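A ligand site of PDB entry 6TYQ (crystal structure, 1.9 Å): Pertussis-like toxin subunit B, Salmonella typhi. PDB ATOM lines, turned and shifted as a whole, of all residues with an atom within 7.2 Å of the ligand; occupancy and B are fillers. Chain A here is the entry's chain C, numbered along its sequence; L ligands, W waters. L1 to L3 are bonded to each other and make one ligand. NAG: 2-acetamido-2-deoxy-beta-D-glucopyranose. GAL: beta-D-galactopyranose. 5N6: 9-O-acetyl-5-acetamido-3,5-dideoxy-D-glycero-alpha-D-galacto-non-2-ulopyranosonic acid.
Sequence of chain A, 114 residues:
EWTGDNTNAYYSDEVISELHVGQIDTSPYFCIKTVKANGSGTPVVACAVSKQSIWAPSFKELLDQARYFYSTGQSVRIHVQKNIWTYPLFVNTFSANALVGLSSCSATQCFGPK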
ATOM      1  N   ASN A   8     -11.048  32.123  12.009  1.00  0.00           N
ATOM      2  CA  ASN A   8     -11.084  31.762  13.410  1.00  0.00           C
ATOM      3  C   ASN A   8     -12.424  31.130  13.764  1.00  0.00           C
ATOM      4  O   ASN A   8     -13.439  31.370  13.100  1.00  0.00           O
ATOM      5  CB  ASN A   8     -10.828  32.984  14.291  1.00  0.00           C
ATOM      6  CG  ASN A   8      -9.448  33.542  14.085  1.00  0.00           C
ATOM      7  OD1 ASN A   8      -8.504  32.796  13.804  1.00  0.00           O
ATOM      8  ND2 ASN A   8      -9.309  34.865  14.211  1.00  0.00           N
ATOM      9  N   ALA A   9     -12.428  30.319  14.818  1.00  0.00           N
ATOM     10  CA  ALA A   9     -13.628  29.617  15.241  1.00  0.00           C
ATOM     11  C   ALA A   9     -14.116  30.209  16.560  1.00  0.00           C
ATOM     12  O   ALA A   9     -13.332  30.769  17.326  1.00  0.00           O
ATOM     13  CB  ALA A   9     -13.361  28.113  15.415  1.00  0.00           C
ATOM     14  N   TYR A  10     -15.414  30.072  16.834  1.00  0.00           N
ATOM     15  CA  TYR A  10     -15.926  30.538  18.119  1.00  0.00           C
ATOM     16  C   TYR A  10     -16.953  29.570  18.683  1.00  0.00           C
ATOM     17  O   TYR A  10     -17.565  28.790  17.961  1.00  0.00           O
ATOM     18  CB  TYR A  10     -16.504  31.955  18.011  1.00  0.00           C
ATOM     19  CG  TYR A  10     -17.745  32.071  17.138  1.00  0.00           C
ATOM     20  CD1 TYR A  10     -19.011  31.837  17.652  1.00  0.00           C
ATOM     21  CD2 TYR A  10     -17.645  32.455  15.800  1.00  0.00           C
ATOM     22  CE1 TYR A  10     -20.154  31.982  16.857  1.00  0.00           C
ATOM     23  CE2 TYR A  10     -18.779  32.586  14.988  1.00  0.00           C
ATOM     24  CZ  TYR A  10     -20.022  32.347  15.530  1.00  0.00           C
ATOM     25  OH  TYR A  10     -21.145  32.474  14.750  1.00  0.00           O
ATOM     26  N   TYR A  11     -17.130  29.655  20.006  1.00  0.00           N
ATOM     27  CA  TYR A  11     -18.019  28.787  20.755  1.00  0.00           C
ATOM     28  C   TYR A  11     -18.745  29.619  21.796  1.00  0.00           C
ATOM     29  O   TYR A  11     -18.096  30.284  22.606  1.00  0.00           O
ATOM     30  CB  TYR A  11     -17.245  27.665  21.439  1.00  0.00           C
ATOM     31  CG  TYR A  11     -16.405  26.852  20.481  1.00  0.00           C
ATOM     32  CD1 TYR A  11     -15.102  27.222  20.188  1.00  0.00           C
ATOM     33  CD2 TYR A  11     -16.928  25.723  19.867  1.00  0.00           C
ATOM     34  CE1 TYR A  11     -14.331  26.477  19.297  1.00  0.00           C
ATOM     35  CE2 TYR A  11     -16.179  24.982  18.977  1.00  0.00           C
ATOM     36  CZ  TYR A  11     -14.872  25.366  18.697  1.00  0.00           C
ATOM     37  OH  TYR A  11     -14.141  24.620  17.819  1.00  0.00           O
ATOM     38  N   SER A  12     -20.078  29.541  21.815  1.00  0.00           N
ATOM     39  CA  SER A  12     -20.916  30.428  22.612  1.00  0.00           C
ATOM     40  C   SER A  12     -21.497  29.703  23.815  1.00  0.00           C
ATOM     41  O   SER A  12     -21.542  28.473  23.880  1.00  0.00           O
ATOM     42  CB  SER A  12     -22.055  30.975  21.730  1.00  0.00           C
ATOM     43  OG  SER A  12     -21.518  31.605  20.570  1.00  0.00           O
ATOM     44  N   ASP A  13     -21.971  30.493  24.784  1.00  0.00           N
ATOM     45  CA  ASP A  13     -22.656  29.975  25.969  1.00  0.00           C
ATOM     46  C   ASP A  13     -21.776  29.008  26.739  1.00  0.00           C
ATOM     47  O   ASP A  13     -22.237  27.971  27.216  1.00  0.00           O
ATOM     48  CB  ASP A  13     -23.985  29.322  25.591  1.00  0.00           C
ATOM     49  CG  ASP A  13     -24.821  30.209  24.698  1.00  0.00           C
ATOM     50  OD1 ASP A  13     -25.144  29.775  23.562  1.00  0.00           O
ATOM     51  OD2 ASP A  13     -25.136  31.349  25.117  1.00  0.00           O
ATOM     52  N   GLU A  14     -20.502  29.346  26.829  1.00  0.00           N
ATOM     53  CA  GLU A  14     -19.490  28.535  27.506  1.00  0.00           C
ATOM     54  C   GLU A  14     -19.197  29.135  28.864  1.00  0.00           C
ATOM     55  O   GLU A  14     -19.346  30.342  29.082  1.00  0.00           O
ATOM     56  CB  GLU A  14     -18.192  28.478  26.699  1.00  0.00           C
ATOM     57  CG  GLU A  14     -18.336  27.953  25.275  1.00  0.00           C
ATOM     58  CD  GLU A  14     -18.304  26.444  25.217  1.00  0.00           C
ATOM     59  OE1 GLU A  14     -17.859  25.811  26.199  1.00  0.00           O
ATOM     60  OE2 GLU A  14     -18.739  25.900  24.192  1.00  0.00           O
ATOM     61  N   THR A  34     -13.311  25.284  28.774  1.00  0.00           N
ATOM     62  CA  THR A  34     -14.675  25.800  28.885  1.00  0.00           C
ATOM     63  C   THR A  34     -15.658  24.687  28.555  1.00  0.00           C
ATOM     64  O   THR A  34     -15.371  23.792  27.746  1.00  0.00           O
ATOM     65  CB  THR A  34     -14.921  27.006  27.950  1.00  0.00           C
ATOM     66  OG1 THR A  34     -15.037  26.575  26.597  1.00  0.00           O
ATOM     67  CG2 THR A  34     -13.790  28.041  28.063  1.00  0.00           C
ATOM     68  N   LYS A  36     -20.139  24.039  28.085  1.00  0.00           N
ATOM     69  CA  LYS A  36     -21.434  24.690  27.900  1.00  0.00           C
ATOM     70  C   LYS A  36     -22.110  24.901  29.243  1.00  0.00           C
ATOM     71  O   LYS A  36     -22.122  23.997  30.098  1.00  0.00           O
ATOM     72  CB  LYS A  36     -22.332  23.864  26.992  1.00  0.00           C
ATOM     73  CG  LYS A  36     -21.846  23.775  25.567  1.00  0.00           C
ATOM     74  CD  LYS A  36     -22.147  25.044  24.792  1.00  0.00           C
ATOM     75  CE  LYS A  36     -21.835  24.834  23.325  1.00  0.00           C
ATOM     76  NZ  LYS A  36     -21.767  26.129  22.597  1.00  0.00           N
ATOM     77  N   ASN A  38     -25.114  24.824  29.983  1.00  0.00           N
ATOM     78  CA  ASN A  38     -26.201  23.884  30.210  1.00  0.00           C
ATOM     79  C   ASN A  38     -25.759  22.433  30.166  1.00  0.00           C
ATOM     80  O   ASN A  38     -26.604  21.525  30.194  1.00  0.00           O
ATOM     81  CB  ASN A  38     -27.319  24.128  29.189  1.00  0.00           C
ATOM     82  CG  ASN A  38     -26.960  23.665  27.794  1.00  0.00           C
ATOM     83  OD1 ASN A  38     -25.847  23.190  27.541  1.00  0.00           O
ATOM     84  ND2 ASN A  38     -27.905  23.788  26.873  1.00  0.00           N
ATOM     85  N   SER A  40     -24.338  20.706  27.719  1.00  0.00           N
ATOM     86  CA  SER A  40     -24.299  20.063  26.405  1.00  0.00           C
ATOM     87  C   SER A  40     -22.876  20.115  25.836  1.00  0.00           C
ATOM     88  O   SER A  40     -21.918  20.505  26.512  1.00  0.00           O
ATOM     89  CB  SER A  40     -25.313  20.717  25.475  1.00  0.00           C
ATOM     90  OG  SER A  40     -25.060  22.092  25.323  1.00  0.00           O
ATOM     91  N   GLY A  41     -22.714  19.722  24.573  1.00  0.00           N
ATOM     92  CA  GLY A  41     -21.490  19.872  23.798  1.00  0.00           C
ATOM     93  C   GLY A  41     -20.296  19.090  24.345  1.00  0.00           C
ATOM     94  O   GLY A  41     -20.423  18.211  25.190  1.00  0.00           O
ATOM     95  N   THR A  42     -19.120  19.442  23.832  1.00  0.00           N
ATOM     96  CA  THR A  42     -17.824  18.907  24.240  1.00  0.00           C
ATOM     97  C   THR A  42     -16.907  20.039  24.720  1.00  0.00           C
ATOM     98  O   THR A  42     -16.977  21.153  24.206  1.00  0.00           O
ATOM     99  CB  THR A  42     -17.132  18.170  23.070  1.00  0.00           C
ATOM    100  OG1 THR A  42     -16.990  19.071  21.967  1.00  0.00           O
ATOM    101  CG2 THR A  42     -17.924  16.950  22.637  1.00  0.00           C
ATOM    102  N   PRO A  43     -16.063  19.781  25.715  1.00  0.00           N
ATOM    103  CA  PRO A  43     -15.229  20.867  26.257  1.00  0.00           C
ATOM    104  C   PRO A  43     -14.345  21.512  25.193  1.00  0.00           C
ATOM    105  O   PRO A  43     -13.924  20.867  24.230  1.00  0.00           O
ATOM    106  CB  PRO A  43     -14.393  20.151  27.326  1.00  0.00           C
ATOM    107  CG  PRO A  43     -15.202  18.943  27.698  1.00  0.00           C
ATOM    108  CD  PRO A  43     -15.837  18.503  26.415  1.00  0.00           C
ATOM    109  N   VAL A  44     -14.103  22.810  25.363  1.00  0.00           N
ATOM    110  CA  VAL A  44     -13.203  23.560  24.498  1.00  0.00           C
ATOM    111  C   VAL A  44     -11.987  23.931  25.335  1.00  0.00           C
ATOM    112  O   VAL A  44     -12.131  24.357  26.493  1.00  0.00           O
ATOM    113  CB  VAL A  44     -13.870  24.813  23.926  1.00  0.00           C
ATOM    114  CG1 VAL A  44     -12.854  25.622  23.129  1.00  0.00           C
ATOM    115  CG2 VAL A  44     -15.070  24.440  23.070  1.00  0.00           C
ATOM    116  N   ARG A  77     -18.347  33.781  25.109  1.00  0.00           N
ATOM    117  CA  ARG A  77     -17.943  33.231  23.829  1.00  0.00           C
ATOM    118  C   ARG A  77     -16.422  33.208  23.792  1.00  0.00           C
ATOM    119  O   ARG A  77     -15.774  34.219  24.089  1.00  0.00           O
ATOM    120  CB  ARG A  77     -18.479  34.055  22.657  1.00  0.00           C
ATOM    121  CG  ARG A  77     -18.073  33.517  21.287  1.00  0.00           C
ATOM    122  CD  ARG A  77     -18.731  34.333  20.176  1.00  0.00           C
ATOM    123  NE  ARG A  77     -20.140  33.997  20.031  1.00  0.00           N
ATOM    124  CZ  ARG A  77     -20.985  34.657  19.244  1.00  0.00           C
ATOM    125  NH1 ARG A  77     -20.566  35.675  18.510  1.00  0.00           N
ATOM    126  NH2 ARG A  77     -22.251  34.283  19.178  1.00  0.00           N
ATOM    127  N   VAL A  80     -11.052  31.252  18.952  1.00  0.00           N
ATOM    128  CA  VAL A  80      -9.785  30.538  18.832  1.00  0.00           C
ATOM    129  C   VAL A  80      -9.330  30.483  17.378  1.00  0.00           C
ATOM    130  O   VAL A  80     -10.137  30.567  16.445  1.00  0.00           O
ATOM    131  CB  VAL A  80      -9.852  29.080  19.390  1.00  0.00           C
ATOM    132  CG1 VAL A  80     -10.404  29.068  20.810  1.00  0.00           C
ATOM    133  CG2 VAL A  80     -10.674  28.184  18.462  1.00  0.00           C
ATOM    134  N   LYS A  82      -7.418  27.538  15.270  1.00  0.00           N
ATOM    135  CA  LYS A  82      -7.034  26.155  15.473  1.00  0.00           C
ATOM    136  C   LYS A  82      -5.652  25.879  14.902  1.00  0.00           C
ATOM    137  O   LYS A  82      -5.122  26.641  14.086  1.00  0.00           O
ATOM    138  CB  LYS A  82      -8.060  25.233  14.817  1.00  0.00           C
ATOM    139  CG  LYS A  82      -9.480  25.541  15.240  1.00  0.00           C
ATOM    140  CD  LYS A  82     -10.465  24.596  14.600  1.00  0.00           C
ATOM    141  CE  LYS A  82     -11.620  24.291  15.545  1.00  0.00           C
ATOM    142  NZ  LYS A  82     -12.448  23.176  14.972  1.00  0.00           N
ATOM    143  N   CYS A 110     -23.783  36.963  23.485  1.00  0.00           N
ATOM    144  CA  CYS A 110     -22.432  36.993  22.948  1.00  0.00           C
ATOM    145  C   CYS A 110     -22.185  38.263  22.149  1.00  0.00           C
ATOM    146  O   CYS A 110     -22.668  38.469  21.028  1.00  0.00           O
ATOM    147  CB  CYS A 110     -22.182  35.711  22.170  1.00  0.00           C
ATOM    148  SG  CYS A 110     -22.577  34.299  23.202  1.00  0.00           S
ATOM    149  N   LYS A 114     -19.048  37.114  14.766  1.00  0.00           N
ATOM    150  CA  LYS A 114     -20.208  36.298  14.569  1.00  0.00           C
ATOM    151  C   LYS A 114     -20.163  35.713  13.158  1.00  0.00           C
ATOM    152  O   LYS A 114     -20.346  36.422  12.166  1.00  0.00           O
ATOM    153  CB  LYS A 114     -21.460  37.146  14.794  1.00  0.00           C
ATOM    154  CG  LYS A 114     -22.502  36.519  15.685  1.00  0.00           C
ATOM    155  CD  LYS A 114     -23.449  35.620  14.904  1.00  0.00           C
ATOM    156  CE  LYS A 114     -24.488  34.993  15.824  1.00  0.00           C
ATOM    157  NZ  LYS A 114     -25.269  33.920  15.145  1.00  0.00           N
HETATM  158  C1  NAG L   1     -25.922  21.332  14.547  1.00  0.00           C
HETATM  159  C2  NAG L   1     -26.899  21.316  15.696  1.00  0.00           C
HETATM  160  C3  NAG L   1     -27.572  22.665  15.755  1.00  0.00           C
HETATM  161  C4  NAG L   1     -26.599  23.741  16.052  1.00  0.00           C
HETATM  162  C5  NAG L   1     -25.472  23.806  15.033  1.00  0.00           C
HETATM  163  C6  NAG L   1     -24.389  24.703  15.485  1.00  0.00           C
HETATM  164  C7  NAG L   1     -28.765  20.167  14.423  1.00  0.00           C
HETATM  165  C8  NAG L   1     -29.735  18.958  14.321  1.00  0.00           C
HETATM  166  N2  NAG L   1     -27.867  20.202  15.533  1.00  0.00           N
HETATM  167  O1  NAG L   1     -25.212  20.163  14.398  1.00  0.00           O
HETATM  168  O3  NAG L   1     -28.574  22.692  16.802  1.00  0.00           O
HETATM  169  O4  NAG L   1     -27.243  25.041  15.942  1.00  0.00           O
HETATM  170  O5  NAG L   1     -24.935  22.451  14.699  1.00  0.00           O
HETATM  171  O6  NAG L   1     -23.801  24.203  16.721  1.00  0.00           O
HETATM  172  O7  NAG L   1     -28.777  21.030  13.606  1.00  0.00           O
HETATM  173  C1  GAL L   2     -27.226  25.935  17.017  1.00  0.00           C
HETATM  174  C2  GAL L   2     -27.978  25.393  18.249  1.00  0.00           C
HETATM  175  C3  GAL L   2     -27.922  26.341  19.405  1.00  0.00           C
HETATM  176  C4  GAL L   2     -26.529  26.683  19.855  1.00  0.00           C
HETATM  177  C5  GAL L   2     -25.785  27.272  18.649  1.00  0.00           C
HETATM  178  C6  GAL L   2     -24.315  27.512  18.914  1.00  0.00           C
HETATM  179  O2  GAL L   2     -29.334  25.139  17.874  1.00  0.00           O
HETATM  180  O3  GAL L   2     -28.625  25.751  20.555  1.00  0.00           O
HETATM  181  O4  GAL L   2     -25.816  25.540  20.366  1.00  0.00           O
HETATM  182  O5  GAL L   2     -25.858  26.364  17.437  1.00  0.00           O
HETATM  183  O6  GAL L   2     -23.693  27.982  17.663  1.00  0.00           O
HETATM  184  CAF 5N6 L   3     -17.316  22.074  21.255  1.00  0.00           C
HETATM  185  CAG 5N6 L   3     -18.861  22.207  21.052  1.00  0.00           C
HETATM  186  C11 5N6 L   3     -16.289  25.548  15.437  1.00  0.00           C
HETATM  187  C10 5N6 L   3     -17.834  25.603  15.491  1.00  0.00           C
HETATM  188  C9  5N6 L   3     -20.736  23.056  19.739  1.00  0.00           C
HETATM  189  C8  5N6 L   3     -21.053  24.458  19.158  1.00  0.00           C
HETATM  190  C7  5N6 L   3     -20.219  24.764  17.892  1.00  0.00           C
HETATM  191  N5  5N6 L   3     -18.478  26.687  16.255  1.00  0.00           N
HETATM  192  C5  5N6 L   3     -19.940  26.767  16.318  1.00  0.00           C
HETATM  193  C4  5N6 L   3     -20.310  28.209  16.167  1.00  0.00           C
HETATM  194  C6  5N6 L   3     -20.339  26.262  17.665  1.00  0.00           C
HETATM  195  C3  5N6 L   3     -21.746  28.539  16.324  1.00  0.00           C
HETATM  196  C2  5N6 L   3     -22.254  27.974  17.648  1.00  0.00           C
HETATM  197  C1  5N6 L   3     -21.805  28.793  18.804  1.00  0.00           C
HETATM  198  OBJ 5N6 L   3     -19.589  21.587  21.736  1.00  0.00           O
HETATM  199  O9  5N6 L   3     -19.352  23.111  20.054  1.00  0.00           O
HETATM  200  O10 5N6 L   3     -18.524  24.801  14.925  1.00  0.00           O
HETATM  201  O7  5N6 L   3     -20.757  24.048  16.815  1.00  0.00           O
HETATM  202  O8  5N6 L   3     -20.802  25.401  20.155  1.00  0.00           O
HETATM  203  O4  5N6 L   3     -19.857  28.652  14.874  1.00  0.00           O
HETATM  204  O6  5N6 L   3     -21.817  26.568  17.831  1.00  0.00           O
HETATM  205  O1B 5N6 L   3     -21.376  28.238  19.857  1.00  0.00           O
HETATM  206  O1A 5N6 L   3     -21.886  30.048  18.764  1.00  0.00           O
HETATM  207  O   HOH W   1     -24.691  23.577  19.131  1.00  0.00           O
HETATM  208  O   HOH W   2     -17.048  29.271  14.409  1.00  0.00           O
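The side-chain hydroxyl of Ser 12 is in hydrogen-bond range of an oxygen (O1A) of 5N6 L3, 2.4 Å away. The backbone NH of Ser 12 sits at hydrogen-bond distance from an oxygen (O1B) of 5N6 L3. The backbone NH (N) of Thr 42 lies within hydrogen-bond range of an oxygen (OBJ) of 5N6 L3, 3.0 Å away. The backbone carbonyl oxygen (O) of Tyr 10 sits at hydrogen-bond distance from a nitrogen (N5) of 5N6 L3 (2.9 Å). NZ of Lys 36 lies within salt-bridge range of O1B of 5N6 L3, 3.5 Å away.
The guanidinium group (NE) of Arg 77 sits at hydrogen-bond distance from the side-chain hydroxyl (OG) of Ser 12, 2.8 Å away. O of Ser 12 sits at hydrogen-bond distance from NZ of Lys 36, 2.7 Å away. The side-chain amino group (NZ) of Lys 36 is in salt-bridge range of the side-chain carboxylate (OE2) of Glu 14 (3.4 Å). The backbone NH (N) of Ala 9 sits at hydrogen-bond distance from the backbone carbonyl oxygen (O) of Val 80 (2.8 Å). O of Val 44 is in hydrogen-bond range of N of Thr 34 (2.7 Å).
Water W2 bridges an oxygen (O4) of 5N6 L3 and the backbone NH of Tyr 10.
CB of Ala 9 touches C11 of 5N6 L3 (3.9 Å). OH of Tyr 11 touches C11 of 5N6 L3, at 3.3 Å. CA of Gly 41 touches OBJ of 5N6 L3, 3.3 Å away. Val 44 touches the ligand. Hydrophobic or aromatic side chains that line the ligand: Ala 9, Tyr 10, Tyr 11 and Val 44. Of the 20 residues printed, 8 come within 4 Å of the ligand. Along chain A the residues within 4 Å of the ligand span positions 9 to 44.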
